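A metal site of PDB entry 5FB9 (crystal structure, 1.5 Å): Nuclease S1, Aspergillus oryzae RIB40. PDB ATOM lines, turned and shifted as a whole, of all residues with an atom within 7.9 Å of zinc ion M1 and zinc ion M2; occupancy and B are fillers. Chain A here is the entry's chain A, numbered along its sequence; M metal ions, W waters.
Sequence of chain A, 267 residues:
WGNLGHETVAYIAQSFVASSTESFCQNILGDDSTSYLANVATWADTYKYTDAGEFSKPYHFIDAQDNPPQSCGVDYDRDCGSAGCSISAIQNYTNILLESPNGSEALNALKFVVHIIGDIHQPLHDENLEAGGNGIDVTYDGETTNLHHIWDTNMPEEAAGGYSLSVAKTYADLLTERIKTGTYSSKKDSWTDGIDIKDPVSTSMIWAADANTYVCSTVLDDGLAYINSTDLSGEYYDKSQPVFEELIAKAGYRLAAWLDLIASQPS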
ATOM      1  N   TRP A   1     -29.802  20.285  10.656  1.00  0.00           N
ATOM      2  CA  TRP A   1     -30.618  21.269   9.833  1.00  0.00           C
ATOM      3  C   TRP A   1     -29.674  22.015   8.938  1.00  0.00           C
ATOM      4  O   TRP A   1     -28.491  22.130   9.197  1.00  0.00           O
ATOM      5  CB  TRP A   1     -31.361  22.314  10.707  1.00  0.00           C
ATOM      6  CG  TRP A   1     -32.141  21.740  11.848  1.00  0.00           C
ATOM      7  CD1 TRP A   1     -31.724  21.657  13.135  1.00  0.00           C
ATOM      8  CD2 TRP A   1     -33.422  21.147  11.819  1.00  0.00           C
ATOM      9  NE1 TRP A   1     -32.663  21.097  13.911  1.00  0.00           N
ATOM     10  CE2 TRP A   1     -33.747  20.762  13.139  1.00  0.00           C
ATOM     11  CE3 TRP A   1     -34.349  20.893  10.813  1.00  0.00           C
ATOM     12  CZ2 TRP A   1     -34.935  20.124  13.462  1.00  0.00           C
ATOM     13  CZ3 TRP A   1     -35.524  20.303  11.134  1.00  0.00           C
ATOM     14  CH2 TRP A   1     -35.815  19.897  12.445  1.00  0.00           C
ATOM     15  N   GLY A   2     -30.269  22.627   7.930  1.00  0.00           N
ATOM     16  CA  GLY A   2     -29.585  23.646   7.123  1.00  0.00           C
ATOM     17  C   GLY A   2     -29.533  24.986   7.853  1.00  0.00           C
ATOM     18  O   GLY A   2     -29.958  25.100   9.029  1.00  0.00           O
ATOM     19  N   ASN A   3     -29.064  26.019   7.159  1.00  0.00           N
ATOM     20  CA  ASN A   3     -28.826  27.291   7.806  1.00  0.00           C
ATOM     21  C   ASN A   3     -30.084  27.923   8.425  1.00  0.00           C
ATOM     22  O   ASN A   3     -30.041  28.416   9.555  1.00  0.00           O
ATOM     23  CB  ASN A   3     -28.221  28.297   6.862  1.00  0.00           C
ATOM     24  CG  ASN A   3     -26.807  27.968   6.470  1.00  0.00           C
ATOM     25  OD1 ASN A   3     -26.188  27.019   6.913  1.00  0.00           O
ATOM     26  ND2 ASN A   3     -26.273  28.838   5.620  1.00  0.00           N
ATOM     27  N   GLY A   5     -32.790  26.455   9.618  1.00  0.00           N
ATOM     28  CA  GLY A   5     -33.126  25.735  10.860  1.00  0.00           C
ATOM     29  C   GLY A   5     -32.234  26.198  12.004  1.00  0.00           C
ATOM     30  O   GLY A   5     -32.750  26.532  13.090  1.00  0.00           O
ATOM     31  N   HIS A   6     -30.931  26.230  11.801  1.00  0.00           N
ATOM     32  CA  HIS A   6     -30.007  26.674  12.852  1.00  0.00           C
ATOM     33  C   HIS A   6     -30.210  28.113  13.330  1.00  0.00           C
ATOM     34  O   HIS A   6     -30.143  28.408  14.519  1.00  0.00           O
ATOM     35  CB  HIS A   6     -28.558  26.437  12.447  1.00  0.00           C
ATOM     36  CG  HIS A   6     -28.217  25.003  12.458  1.00  0.00           C
ATOM     37  ND1 HIS A   6     -28.091  24.312  13.638  1.00  0.00           N
ATOM     38  CD2 HIS A   6     -28.141  24.067  11.482  1.00  0.00           C
ATOM     39  CE1 HIS A   6     -27.894  23.033  13.400  1.00  0.00           C
ATOM     40  NE2 HIS A   6     -27.954  22.840  12.086  1.00  0.00           N
ATOM     41  N   ALA A  41     -24.761  30.594  14.230  1.00  0.00           N
ATOM     42  CA  ALA A  41     -25.428  29.286  14.361  1.00  0.00           C
ATOM     43  C   ALA A  41     -25.098  28.303  13.211  1.00  0.00           C
ATOM     44  O   ALA A  41     -25.295  27.096  13.374  1.00  0.00           O
ATOM     45  CB  ALA A  41     -26.923  29.514  14.484  1.00  0.00           C
ATOM     46  N   THR A  42     -24.570  28.829  12.078  1.00  0.00           N
ATOM     47  CA  THR A  42     -24.190  28.009  10.915  1.00  0.00           C
ATOM     48  C   THR A  42     -22.698  27.741  10.829  1.00  0.00           C
ATOM     49  O   THR A  42     -22.290  26.979   9.978  1.00  0.00           O
ATOM     50  CB  THR A  42     -24.638  28.640   9.583  1.00  0.00           C
ATOM     51  OG1 THR A  42     -23.752  29.739   9.277  1.00  0.00           O
ATOM     52  CG2 THR A  42     -26.062  29.100   9.646  1.00  0.00           C
ATOM     53  N   ALA A  44     -20.536  25.918  12.387  1.00  0.00           N
ATOM     54  CA  ALA A  44     -20.030  24.538  12.461  1.00  0.00           C
ATOM     55  C   ALA A  44     -20.191  23.849  11.106  1.00  0.00           C
ATOM     56  O   ALA A  44     -19.417  22.978  10.765  1.00  0.00           O
ATOM     57  CB  ALA A  44     -20.723  23.748  13.554  1.00  0.00           C
ATOM     58  N   ASP A  45     -21.215  24.243  10.354  1.00  0.00           N
ATOM     59  CA  ASP A  45     -21.468  23.629   9.062  1.00  0.00           C
ATOM     60  C   ASP A  45     -20.518  24.116   7.976  1.00  0.00           C
ATOM     61  O   ASP A  45     -20.475  23.477   6.915  1.00  0.00           O
ATOM     62  CB  ASP A  45     -22.953  23.800   8.611  1.00  0.00           C
ATOM     63  CG  ASP A  45     -23.885  22.710   9.177  1.00  0.00           C
ATOM     64  OD1 ASP A  45     -23.374  21.725   9.774  1.00  0.00           O
ATOM     65  OD2 ASP A  45     -25.108  22.841   9.027  1.00  0.00           O
ATOM     66  N   THR A  46     -19.907  25.262   8.160  1.00  0.00           N
ATOM     67  CA  THR A  46     -18.822  25.684   7.239  1.00  0.00           C
ATOM     68  C   THR A  46     -17.491  25.130   7.698  1.00  0.00           C
ATOM     69  O   THR A  46     -16.728  24.620   6.883  1.00  0.00           O
ATOM     70  CB  THR A  46     -18.767  27.185   7.097  1.00  0.00           C
ATOM     71  OG1 THR A  46     -20.060  27.601   6.640  1.00  0.00           O
ATOM     72  CG2 THR A  46     -17.754  27.577   6.055  1.00  0.00           C
ATOM     73  N   LYS A  48     -16.688  22.387   9.145  1.00  0.00           N
ATOM     74  CA  LYS A  48     -16.500  20.960   8.911  1.00  0.00           C
ATOM     75  C   LYS A  48     -15.935  20.610   7.531  1.00  0.00           C
ATOM     76  O   LYS A  48     -15.519  19.498   7.330  1.00  0.00           O
ATOM     77  CB  LYS A  48     -17.789  20.191   9.175  1.00  0.00           C
ATOM     78  CG  LYS A  48     -18.861  20.392   8.129  1.00  0.00           C
ATOM     79  CD  LYS A  48     -20.194  19.780   8.571  1.00  0.00           C
ATOM     80  CE  LYS A  48     -21.303  19.969   7.559  1.00  0.00           C
ATOM     81  NZ  LYS A  48     -22.622  19.485   8.072  1.00  0.00           N
ATOM     82  N   SER A  56     -14.558  17.514  13.191  1.00  0.00           N
ATOM     83  CA  SER A  56     -15.813  17.869  13.858  1.00  0.00           C
ATOM     84  C   SER A  56     -17.032  17.453  13.073  1.00  0.00           C
ATOM     85  O   SER A  56     -18.157  17.611  13.569  1.00  0.00           O
ATOM     86  CB  SER A  56     -15.856  19.348  14.146  1.00  0.00           C
ATOM     87  OG  SER A  56     -16.058  20.170  12.985  1.00  0.00           O
ATOM     88  N   LYS A  57     -16.864  16.906  11.867  1.00  0.00           N
ATOM     89  CA  LYS A  57     -18.003  16.339  11.139  1.00  0.00           C
ATOM     90  C   LYS A  57     -18.942  15.404  11.958  1.00  0.00           C
ATOM     91  O   LYS A  57     -20.164  15.519  11.917  1.00  0.00           O
ATOM     92  CB  LYS A  57     -17.534  15.587   9.891  1.00  0.00           C
ATOM     93  CG  LYS A  57     -17.013  16.486   8.791  1.00  0.00           C
ATOM     94  CD  LYS A  57     -16.256  15.703   7.708  1.00  0.00           C
ATOM     95  CE  LYS A  57     -17.062  14.525   7.169  1.00  0.00           C
ATOM     96  NZ  LYS A  57     -16.389  13.720   6.092  1.00  0.00           N
ATOM     97  N   TYR A  59     -19.599  15.333  14.960  1.00  0.00           N
ATOM     98  CA  TYR A  59     -20.227  16.033  16.069  1.00  0.00           C
ATOM     99  C   TYR A  59     -21.643  16.549  15.755  1.00  0.00           C
ATOM    100  O   TYR A  59     -22.298  17.022  16.655  1.00  0.00           O
ATOM    101  CB  TYR A  59     -19.365  17.193  16.577  1.00  0.00           C
ATOM    102  CG  TYR A  59     -17.947  16.841  17.025  1.00  0.00           C
ATOM    103  CD1 TYR A  59     -17.527  15.514  17.238  1.00  0.00           C
ATOM    104  CD2 TYR A  59     -17.075  17.840  17.346  1.00  0.00           C
ATOM    105  CE1 TYR A  59     -16.246  15.210  17.660  1.00  0.00           C
ATOM    106  CE2 TYR A  59     -15.780  17.545  17.757  1.00  0.00           C
ATOM    107  CZ  TYR A  59     -15.399  16.255  17.917  1.00  0.00           C
ATOM    108  OH  TYR A  59     -14.089  16.016  18.383  1.00  0.00           O
ATOM    109  N   HIS A  60     -22.125  16.368  14.529  1.00  0.00           N
ATOM    110  CA  HIS A  60     -23.466  16.799  14.193  1.00  0.00           C
ATOM    111  C   HIS A  60     -24.511  15.701  14.415  1.00  0.00           C
ATOM    112  O   HIS A  60     -25.725  15.969  14.286  1.00  0.00           O
ATOM    113  CB  HIS A  60     -23.438  17.259  12.727  1.00  0.00           C
ATOM    114  CG  HIS A  60     -22.541  18.418  12.494  1.00  0.00           C
ATOM    115  ND1 HIS A  60     -22.993  19.634  12.061  1.00  0.00           N
ATOM    116  CD2 HIS A  60     -21.224  18.563  12.727  1.00  0.00           C
ATOM    117  CE1 HIS A  60     -21.978  20.487  12.025  1.00  0.00           C
ATOM    118  NE2 HIS A  60     -20.895  19.859  12.427  1.00  0.00           N
ATOM    119  N   PHE A  61     -24.054  14.508  14.749  1.00  0.00           N
ATOM    120  CA  PHE A  61     -24.875  13.295  14.712  1.00  0.00           C
ATOM    121  C   PHE A  61     -24.699  12.430  15.932  1.00  0.00           C
ATOM    122  O   PHE A  61     -23.603  12.402  16.497  1.00  0.00           O
ATOM    123  CB  PHE A  61     -24.473  12.376  13.506  1.00  0.00           C
ATOM    124  CG  PHE A  61     -24.356  13.081  12.164  1.00  0.00           C
ATOM    125  CD1 PHE A  61     -25.519  13.511  11.512  1.00  0.00           C
ATOM    126  CD2 PHE A  61     -23.151  13.315  11.578  1.00  0.00           C
ATOM    127  CE1 PHE A  61     -25.442  14.148  10.279  1.00  0.00           C
ATOM    128  CE2 PHE A  61     -23.042  13.964  10.358  1.00  0.00           C
ATOM    129  CZ  PHE A  61     -24.200  14.376   9.699  1.00  0.00           C
ATOM    130  N   HIS A 115     -24.989  25.418  17.651  1.00  0.00           N
ATOM    131  CA  HIS A 115     -25.312  24.581  16.477  1.00  0.00           C
ATOM    132  C   HIS A 115     -25.813  23.213  16.829  1.00  0.00           C
ATOM    133  O   HIS A 115     -26.819  22.731  16.302  1.00  0.00           O
ATOM    134  CB  HIS A 115     -24.053  24.474  15.579  1.00  0.00           C
ATOM    135  CG  HIS A 115     -24.286  23.753  14.286  1.00  0.00           C
ATOM    136  ND1 HIS A 115     -24.744  24.386  13.148  1.00  0.00           N
ATOM    137  CD2 HIS A 115     -24.164  22.447  13.974  1.00  0.00           C
ATOM    138  CE1 HIS A 115     -24.862  23.480  12.184  1.00  0.00           C
ATOM    139  NE2 HIS A 115     -24.586  22.292  12.667  1.00  0.00           N
ATOM    140  N   ILE A 116     -25.074  22.548  17.699  1.00  0.00           N
ATOM    141  CA  ILE A 116     -25.264  21.111  17.930  1.00  0.00           C
ATOM    142  C   ILE A 116     -26.540  20.896  18.717  1.00  0.00           C
ATOM    143  O   ILE A 116     -27.237  19.894  18.465  1.00  0.00           O
ATOM    144  CB  ILE A 116     -24.016  20.463  18.563  1.00  0.00           C
ATOM    145  CG1 ILE A 116     -22.839  20.564  17.579  1.00  0.00           C
ATOM    146  CG2 ILE A 116     -24.340  19.042  18.971  1.00  0.00           C
ATOM    147  CD1 ILE A 116     -21.522  20.088  18.211  1.00  0.00           C
ATOM    148  N   GLY A 118     -29.157  22.510  18.192  1.00  0.00           N
ATOM    149  CA  GLY A 118     -30.052  22.428  17.039  1.00  0.00           C
ATOM    150  C   GLY A 118     -30.056  21.031  16.362  1.00  0.00           C
ATOM    151  O   GLY A 118     -31.123  20.421  16.148  1.00  0.00           O
ATOM    152  N   ASP A 119     -28.861  20.519  15.973  1.00  0.00           N
ATOM    153  CA  ASP A 119     -28.796  19.226  15.295  1.00  0.00           C
ATOM    154  C   ASP A 119     -29.368  18.046  16.070  1.00  0.00           C
ATOM    155  O   ASP A 119     -29.999  17.187  15.502  1.00  0.00           O
ATOM    156  CB  ASP A 119     -27.375  18.913  14.871  1.00  0.00           C
ATOM    157  CG  ASP A 119     -27.015  19.531  13.569  1.00  0.00           C
ATOM    158  OD1 ASP A 119     -27.878  19.960  12.795  1.00  0.00           O
ATOM    159  OD2 ASP A 119     -25.797  19.585  13.299  1.00  0.00           O
ATOM    160  N   ILE A 120     -29.213  18.036  17.388  1.00  0.00           N
ATOM    161  CA  ILE A 120     -29.782  16.963  18.225  1.00  0.00           C
ATOM    162  C   ILE A 120     -31.285  16.861  18.056  1.00  0.00           C
ATOM    163  O   ILE A 120     -31.890  15.809  18.269  1.00  0.00           O
ATOM    164  CB  ILE A 120     -29.348  17.174  19.688  1.00  0.00           C
ATOM    165  CG1 ILE A 120     -27.851  16.848  19.839  1.00  0.00           C
ATOM    166  CG2 ILE A 120     -30.168  16.331  20.611  1.00  0.00           C
ATOM    167  CD1 ILE A 120     -27.253  17.372  21.155  1.00  0.00           C
ATOM    168  N   GLN A 122     -32.933  17.413  15.160  1.00  0.00           N
ATOM    169  CA  GLN A 122     -33.302  16.957  13.806  1.00  0.00           C
ATOM    170  C   GLN A 122     -33.332  15.456  13.909  1.00  0.00           C
ATOM    171  O   GLN A 122     -32.247  14.874  14.107  1.00  0.00           O
ATOM    172  CB  GLN A 122     -32.292  17.521  12.777  1.00  0.00           C
ATOM    173  CG  GLN A 122     -32.787  17.705  11.349  1.00  0.00           C
ATOM    174  CD  GLN A 122     -33.051  16.433  10.586  1.00  0.00           C
ATOM    175  OE1 GLN A 122     -33.799  15.572  11.052  1.00  0.00           O
ATOM    176  NE2 GLN A 122     -32.466  16.286   9.389  1.00  0.00           N
ATOM    177  N   HIS A 125     -30.655  13.413  12.298  1.00  0.00           N
ATOM    178  CA  HIS A 125     -29.340  13.545  12.912  1.00  0.00           C
ATOM    179  C   HIS A 125     -29.119  12.579  14.080  1.00  0.00           C
ATOM    180  O   HIS A 125     -28.008  12.519  14.623  1.00  0.00           O
ATOM    181  CB  HIS A 125     -29.069  14.978  13.337  1.00  0.00           C
ATOM    182  CG  HIS A 125     -28.598  15.850  12.224  1.00  0.00           C
ATOM    183  ND1 HIS A 125     -27.376  16.463  12.231  1.00  0.00           N
ATOM    184  CD2 HIS A 125     -29.176  16.172  11.049  1.00  0.00           C
ATOM    185  CE1 HIS A 125     -27.187  17.082  11.067  1.00  0.00           C
ATOM    186  NE2 HIS A 125     -28.278  16.951  10.362  1.00  0.00           N
ATOM    187  N   HIS A 148     -32.949  12.744   4.271  1.00  0.00           N
ATOM    188  CA  HIS A 148     -32.256  13.608   5.189  1.00  0.00           C
ATOM    189  C   HIS A 148     -32.367  15.074   4.791  1.00  0.00           C
ATOM    190  O   HIS A 148     -32.684  15.937   5.633  1.00  0.00           O
ATOM    191  CB  HIS A 148     -30.760  13.192   5.292  1.00  0.00           C
ATOM    192  CG  HIS A 148     -30.029  13.891   6.376  1.00  0.00           C
ATOM    193  ND1 HIS A 148     -29.773  13.326   7.613  1.00  0.00           N
ATOM    194  CD2 HIS A 148     -29.563  15.141   6.428  1.00  0.00           C
ATOM    195  CE1 HIS A 148     -29.167  14.230   8.370  1.00  0.00           C
ATOM    196  NE2 HIS A 148     -29.035  15.331   7.681  1.00  0.00           N
ATOM    197  N   ASP A 152     -33.663  18.503   6.681  1.00  0.00           N
ATOM    198  CA  ASP A 152     -32.728  19.547   7.007  1.00  0.00           C
ATOM    199  C   ASP A 152     -33.191  20.891   6.430  1.00  0.00           C
ATOM    200  O   ASP A 152     -32.988  21.936   7.046  1.00  0.00           O
ATOM    201  CB  ASP A 152     -31.302  19.279   6.433  1.00  0.00           C
ATOM    202  CG  ASP A 152     -30.391  18.512   7.368  1.00  0.00           C
ATOM    203  OD1 ASP A 152     -30.665  18.310   8.552  1.00  0.00           O
ATOM    204  OD2 ASP A 152     -29.363  18.118   6.829  1.00  0.00           O
ATOM    205  N   THR A 153     -33.735  20.844   5.224  1.00  0.00           N
ATOM    206  CA  THR A 153     -33.780  21.977   4.347  1.00  0.00           C
ATOM    207  C   THR A 153     -35.120  22.189   3.622  1.00  0.00           C
ATOM    208  O   THR A 153     -35.750  23.213   3.815  1.00  0.00           O
ATOM    209  CB  THR A 153     -32.616  21.883   3.346  1.00  0.00           C
ATOM    210  OG1 THR A 153     -31.367  22.010   4.066  1.00  0.00           O
ATOM    211  CG2 THR A 153     -32.631  22.944   2.268  1.00  0.00           C
HETATM  212 ZN    ZN M   1     -27.921  21.105  11.028  1.00  0.00          ZN
HETATM  213 ZN    ZN M   2     -24.785  20.486  11.707  1.00  0.00          ZN
HETATM  214 ZN    ZN M   3     -28.267  17.215   8.245  1.00  0.00          ZN
HETATM  215  O   HOH W   1     -24.227  17.859   9.471  1.00  0.00           O
HETATM  216  O   HOH W   2     -27.491  19.060   8.468  1.00  0.00           O
HETATM  217  O   HOH W   3     -26.147  20.730  10.416  1.00  0.00           O
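Water W3 is bound to zinc ion M1 (1.9 Å).
A ring nitrogen (NE2) of His 6 binds zinc ion M1, at 2.0 Å.
N of Trp 1 is bound to zinc ion M1 (2.1 Å).
Zinc ion M1 is bound by OD1 of Asp 119 (2.1 Å).
The backbone carbonyl oxygen (O) of Trp 1 binds zinc ion M1 (2.2 Å).
Zinc ion M1 has five donor atoms within binding distance.
Of the 26 residues printed, 5 come within 4 Å of zinc ion M1.
The nearest printed residue that does not touch zinc ion M1 is His 125 (4.1 Å).
Zinc ion M2 is bound by water W3 (1.9 Å), a ring nitrogen (ND1) of His 60 (2.0 Å), a ring nitrogen (NE2) of His 115 (2.1 Å) and the side-chain carboxylate of Asp 119 (2.1 Å).
Slightly farther from zinc ion M2 lies the side-chain carboxylate (OD1) of Asp 45 (2.7 Å).
OD1 of Asp 45 lies close to ND1 of His 60, at 3.1 Å.
The backbone carbonyl oxygen (O) of His 60 sits at hydrogen-bond distance from a ring nitrogen (ND1) of His 125.
The backbone carbonyl oxygen of His 115 sits close to a ring nitrogen (ND1) of His 6, 3.3 Å away.
The side-chain carboxylate (OD1) of Asp 45 sits close to a ring nitrogen (NE2) of His 115.
ND1 of His 115 is in hydrogen-bond range of O of Ala 41, at 2.8 Å.
The backbone NH (N) of Trp 1 lies close to the side-chain carboxylate (OD1) of Asp 152, at 3.0 Å.
NE1 of Trp 1 is in hydrogen-bond range of O of Gly 118, 2.8 Å away.
The side-chain carboxylate (OD1) of Asp 45 is in salt-bridge range of the side-chain amino group (NZ) of Lys 48, 2.9 Å away.
Five residues have an atom within 4 Å of zinc ion M2: His 6, Asp 45, His 60, His 115 and Asp 119.
The nearest printed residue that does not touch zinc ion M2 is His 125 (4.2 Å).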
